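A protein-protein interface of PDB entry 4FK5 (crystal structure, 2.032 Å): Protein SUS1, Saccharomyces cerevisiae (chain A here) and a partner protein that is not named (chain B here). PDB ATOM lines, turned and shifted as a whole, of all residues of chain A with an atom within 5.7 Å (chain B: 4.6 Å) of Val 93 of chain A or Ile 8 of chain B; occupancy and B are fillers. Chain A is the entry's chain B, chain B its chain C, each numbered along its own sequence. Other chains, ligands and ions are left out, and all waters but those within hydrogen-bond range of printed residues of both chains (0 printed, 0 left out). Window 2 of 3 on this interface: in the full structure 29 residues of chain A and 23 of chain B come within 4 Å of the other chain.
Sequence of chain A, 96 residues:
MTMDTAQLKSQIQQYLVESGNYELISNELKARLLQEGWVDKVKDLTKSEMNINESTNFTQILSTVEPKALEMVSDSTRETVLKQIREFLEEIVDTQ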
ATOM      1  N   ILE A  12     -23.950  24.779  26.884  1.00  0.00           N
ATOM      2  CA  ILE A  12     -25.112  23.933  26.516  1.00  0.00           C
ATOM      3  C   ILE A  12     -26.460  24.702  26.723  1.00  0.00           C
ATOM      4  O   ILE A  12     -27.348  24.686  25.855  1.00  0.00           O
ATOM      5  CB  ILE A  12     -25.084  22.608  27.294  1.00  0.00           C
ATOM      6  CG1 ILE A  12     -23.935  21.722  26.751  1.00  0.00           C
ATOM      7  CG2 ILE A  12     -26.446  21.865  27.221  1.00  0.00           C
ATOM      8  CD1 ILE A  12     -23.842  20.374  27.401  1.00  0.00           C
ATOM      9  N   ARG A  86     -32.116  15.141  27.836  1.00  0.00           N
ATOM     10  CA  ARG A  86     -30.995  14.183  27.269  1.00  0.00           C
ATOM     11  C   ARG A  86     -31.028  14.155  25.845  1.00  0.00           C
ATOM     12  O   ARG A  86     -29.991  14.223  25.234  1.00  0.00           O
ATOM     13  CB  ARG A  86     -31.091  12.654  27.659  1.00  0.00           C
ATOM     14  CG  ARG A  86     -29.764  11.883  27.439  1.00  0.00           C
ATOM     15  CD  ARG A  86     -29.867  10.360  27.618  1.00  0.00           C
ATOM     16  NE  ARG A  86     -28.719   9.701  26.951  1.00  0.00           N
ATOM     17  CZ  ARG A  86     -27.634   9.267  27.579  1.00  0.00           C
ATOM     18  NH1 ARG A  86     -27.503   9.421  28.895  1.00  0.00           N
ATOM     19  NH2 ARG A  86     -26.668   8.661  26.890  1.00  0.00           N
ATOM     20  N   LEU A  89     -29.584  17.014  24.253  1.00  0.00           N
ATOM     21  CA  LEU A  89     -28.093  17.051  24.451  1.00  0.00           C
ATOM     22  C   LEU A  89     -27.350  15.985  23.552  1.00  0.00           C
ATOM     23  O   LEU A  89     -26.271  16.255  23.022  1.00  0.00           O
ATOM     24  CB  LEU A  89     -27.691  16.840  25.928  1.00  0.00           C
ATOM     25  CG  LEU A  89     -28.155  17.821  26.987  1.00  0.00           C
ATOM     26  CD1 LEU A  89     -27.221  17.927  28.179  1.00  0.00           C
ATOM     27  CD2 LEU A  89     -28.536  19.190  26.454  1.00  0.00           C
ATOM     28  N   GLU A  90     -27.980  14.826  23.352  1.00  0.00           N
ATOM     29  CA  GLU A  90     -27.448  13.766  22.456  1.00  0.00           C
ATOM     30  C   GLU A  90     -27.130  14.326  21.064  1.00  0.00           C
ATOM     31  O   GLU A  90     -26.190  13.879  20.433  1.00  0.00           O
ATOM     32  CB  GLU A  90     -28.459  12.600  22.299  1.00  0.00           C
ATOM     33  CG  GLU A  90     -28.407  11.519  23.379  1.00  0.00           C
ATOM     34  CD  GLU A  90     -29.698  10.625  23.405  1.00  0.00           C
ATOM     35  OE1 GLU A  90     -30.139  10.250  24.512  1.00  0.00           O
ATOM     36  OE2 GLU A  90     -30.274  10.313  22.307  1.00  0.00           O
ATOM     37  N   GLU A  91     -27.910  15.305  20.606  1.00  0.00           N
ATOM     38  CA  GLU A  91     -27.684  15.919  19.292  1.00  0.00           C
ATOM     39  C   GLU A  91     -26.435  16.780  19.221  1.00  0.00           C
ATOM     40  O   GLU A  91     -25.939  17.030  18.126  1.00  0.00           O
ATOM     41  CB  GLU A  91     -28.904  16.781  18.845  1.00  0.00           C
ATOM     42  CG  GLU A  91     -30.195  16.019  18.747  1.00  0.00           C
ATOM     43  CD  GLU A  91     -31.234  16.721  17.872  1.00  0.00           C
ATOM     44  OE1 GLU A  91     -31.607  17.890  18.178  1.00  0.00           O
ATOM     45  OE2 GLU A  91     -31.724  16.078  16.906  1.00  0.00           O
ATOM     46  N   ILE A  92     -25.959  17.295  20.362  1.00  0.00           N
ATOM     47  CA  ILE A  92     -24.892  18.324  20.343  1.00  0.00           C
ATOM     48  C   ILE A  92     -23.599  17.984  21.106  1.00  0.00           C
ATOM     49  O   ILE A  92     -22.641  18.786  21.070  1.00  0.00           O
ATOM     50  CB  ILE A  92     -25.379  19.703  20.828  1.00  0.00           C
ATOM     51  CG1 ILE A  92     -25.673  19.682  22.347  1.00  0.00           C
ATOM     52  CG2 ILE A  92     -26.595  20.151  19.997  1.00  0.00           C
ATOM     53  CD1 ILE A  92     -25.572  21.029  23.010  1.00  0.00           C
ATOM     54  N   VAL A  93     -23.565  16.868  21.827  1.00  0.00           N
ATOM     55  CA  VAL A  93     -22.369  16.538  22.593  1.00  0.00           C
ATOM     56  C   VAL A  93     -21.719  15.250  22.049  1.00  0.00           C
ATOM     57  O   VAL A  93     -22.415  14.306  21.612  1.00  0.00           O
ATOM     58  CB  VAL A  93     -22.618  16.431  24.177  1.00  0.00           C
ATOM     59  CG1 VAL A  93     -23.559  17.517  24.689  1.00  0.00           C
ATOM     60  CG2 VAL A  93     -23.114  15.071  24.566  1.00  0.00           C
ATOM     61  N   ASP A  94     -20.400  15.224  22.054  1.00  0.00           N
ATOM     62  CA  ASP A  94     -19.664  13.972  21.797  1.00  0.00           C
ATOM     63  C   ASP A  94     -19.339  13.313  23.110  1.00  0.00           C
ATOM     64  O   ASP A  94     -19.014  13.998  24.101  1.00  0.00           O
ATOM     65  CB  ASP A  94     -18.373  14.251  21.035  1.00  0.00           C
ATOM     66  CG  ASP A  94     -18.619  14.840  19.692  1.00  0.00           C
ATOM     67  OD1 ASP A  94     -19.479  14.275  18.958  1.00  0.00           O
ATOM     68  OD2 ASP A  94     -17.981  15.890  19.365  1.00  0.00           O
ATOM     69  N   THR A  95     -19.459  11.990  23.131  1.00  0.00           N
ATOM     70  CA  THR A  95     -19.144  11.191  24.321  1.00  0.00           C
ATOM     71  C   THR A  95     -17.974  10.295  24.000  1.00  0.00           C
ATOM     72  O   THR A  95     -17.502  10.263  22.865  1.00  0.00           O
ATOM     73  CB  THR A  95     -20.359  10.316  24.789  1.00  0.00           C
ATOM     74  OG1 THR A  95     -20.619   9.304  23.827  1.00  0.00           O
ATOM     75  CG2 THR A  95     -21.649  11.173  24.982  1.00  0.00           C
ATOM     76  N   THR B   7     -21.347  13.661  32.641  1.00  0.00           N
ATOM     77  CA  THR B   7     -22.059  12.825  31.651  1.00  0.00           C
ATOM     78  C   THR B   7     -23.299  13.555  31.102  1.00  0.00           C
ATOM     79  O   THR B   7     -23.762  14.526  31.694  1.00  0.00           O
ATOM     80  CB  THR B   7     -22.537  11.505  32.282  1.00  0.00           C
ATOM     81  OG1 THR B   7     -23.444  11.781  33.348  1.00  0.00           O
ATOM     82  CG2 THR B   7     -21.306  10.625  32.836  1.00  0.00           C
ATOM     83  N   ILE B   8     -23.883  13.035  30.029  1.00  0.00           N
ATOM     84  CA  ILE B   8     -25.148  13.556  29.560  1.00  0.00           C
ATOM     85  C   ILE B   8     -26.168  13.574  30.657  1.00  0.00           C
ATOM     86  O   ILE B   8     -26.938  14.566  30.802  1.00  0.00           O
ATOM     87  CB  ILE B   8     -25.712  12.816  28.363  1.00  0.00           C
ATOM     88  CG1 ILE B   8     -24.787  12.961  27.202  1.00  0.00           C
ATOM     89  CG2 ILE B   8     -27.101  13.426  27.981  1.00  0.00           C
ATOM     90  CD1 ILE B   8     -25.494  12.998  25.860  1.00  0.00           C
ATOM     91  N   ASP B   9     -26.166  12.531  31.484  1.00  0.00           N
ATOM     92  CA  ASP B   9     -27.138  12.449  32.576  1.00  0.00           C
ATOM     93  C   ASP B   9     -26.885  13.488  33.681  1.00  0.00           C
ATOM     94  O   ASP B   9     -27.838  14.061  34.210  1.00  0.00           O
ATOM     95  CB  ASP B   9     -27.200  11.043  33.171  1.00  0.00           C
ATOM     96  CG  ASP B   9     -28.012  10.074  32.309  1.00  0.00           C
ATOM     97  OD1 ASP B   9     -28.830  10.531  31.451  1.00  0.00           O
ATOM     98  OD2 ASP B   9     -27.824   8.853  32.474  1.00  0.00           O
ATOM     99  N   SER B  10     -25.628  13.738  34.027  1.00  0.00           N
ATOM    100  CA  SER B  10     -25.362  14.685  35.114  1.00  0.00           C
ATOM    101  C   SER B  10     -25.665  16.127  34.677  1.00  0.00           C
ATOM    102  O   SER B  10     -26.211  16.908  35.447  1.00  0.00           O
ATOM    103  CB  SER B  10     -23.940  14.560  35.654  1.00  0.00           C
ATOM    104  OG  SER B  10     -22.982  14.826  34.669  1.00  0.00           O
ATOM    105  N   ILE B  11     -25.360  16.441  33.443  1.00  0.00           N
ATOM    106  CA  ILE B  11     -25.646  17.762  32.886  1.00  0.00           C
ATOM    107  C   ILE B  11     -27.146  17.955  32.775  1.00  0.00           C
ATOM    108  O   ILE B  11     -27.679  18.968  33.220  1.00  0.00           O
ATOM    109  CB  ILE B  11     -24.989  17.965  31.488  1.00  0.00           C
ATOM    110  CG1 ILE B  11     -23.461  17.975  31.581  1.00  0.00           C
ATOM    111  CG2 ILE B  11     -25.421  19.296  30.877  1.00  0.00           C
ATOM    112  CD1 ILE B  11     -22.934  19.090  32.463  1.00  0.00           C
ATOM    113  N   SER B  12     -27.837  16.954  32.221  1.00  0.00           N
ATOM    114  CA  SER B  12     -29.315  16.961  32.194  1.00  0.00           C
ATOM    115  C   SER B  12     -29.951  17.196  33.538  1.00  0.00           C
ATOM    116  O   SER B  12     -30.877  18.031  33.673  1.00  0.00           O
ATOM    117  CB  SER B  12     -29.830  15.660  31.574  1.00  0.00           C
ATOM    118  OG  SER B  12     -29.395  15.594  30.241  1.00  0.00           O
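The guanidinium group (NH1) of Arg 86 of chain A lies within salt-bridge range of the side-chain carboxylate (OD1) of Asp 9 of chain B (3.1 Å).
OG1 of Thr 7 of chain B sits close to N of Asp 9 of chain B.
NE of Arg 86 of chain A is in salt-bridge range of OE1 of Glu 90 of chain A, at 2.9 Å.
OG of Ser 12 of chain B lies within hydrogen-bond range of O of Ile 8 of chain B.
Of the 6 printed residues of chain B, 4 touch a printed residue of chain A.
Hydrophobic or aromatic side chains of chain B that line the printed part of chain A: Ile 8 and Ile 11.
Of the printed residues of chain B, Glu 90 of chain A touches Ile 8 (3.98 Å).
Of chain B, only Ile 8 comes within 4 Å of Val 93 of chain A.
Thr 7 of chain B touches none of the printed residues of chain A.
Of the printed residues of chain A, Ser 12 of chain B touches Arg 86 (3.7 Å) and Leu 89 (3.8 Å).
The nearest printed residue of chain A that does not touch Ile 8 of chain B is Leu 89 of chain A (4.03 Å).
The nearest printed residue of chain A that does not touch Ile 11 of chain B is Val 93 of chain A (6.7 Å).
CG2 of Ile 11 of chain B touches CD1 of Ile 12 of chain A (3.97 Å).
Arg 86 of chain A touches Ile 8 of chain B (CG to CG2, 3.1 Å).
Arg 86 of chain A touches Ser 12 of chain B.
Ile 11 of chain B touches Leu 89 of chain A.
CD1 of Leu 89 of chain A touches OG of Ser 12 of chain B (3.8 Å).
Glu 90 of chain A touches Ile 8 of chain B.
Val 93 of chain A touches Ile 8 of chain B (CG2 to CD1, 3.4 Å).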
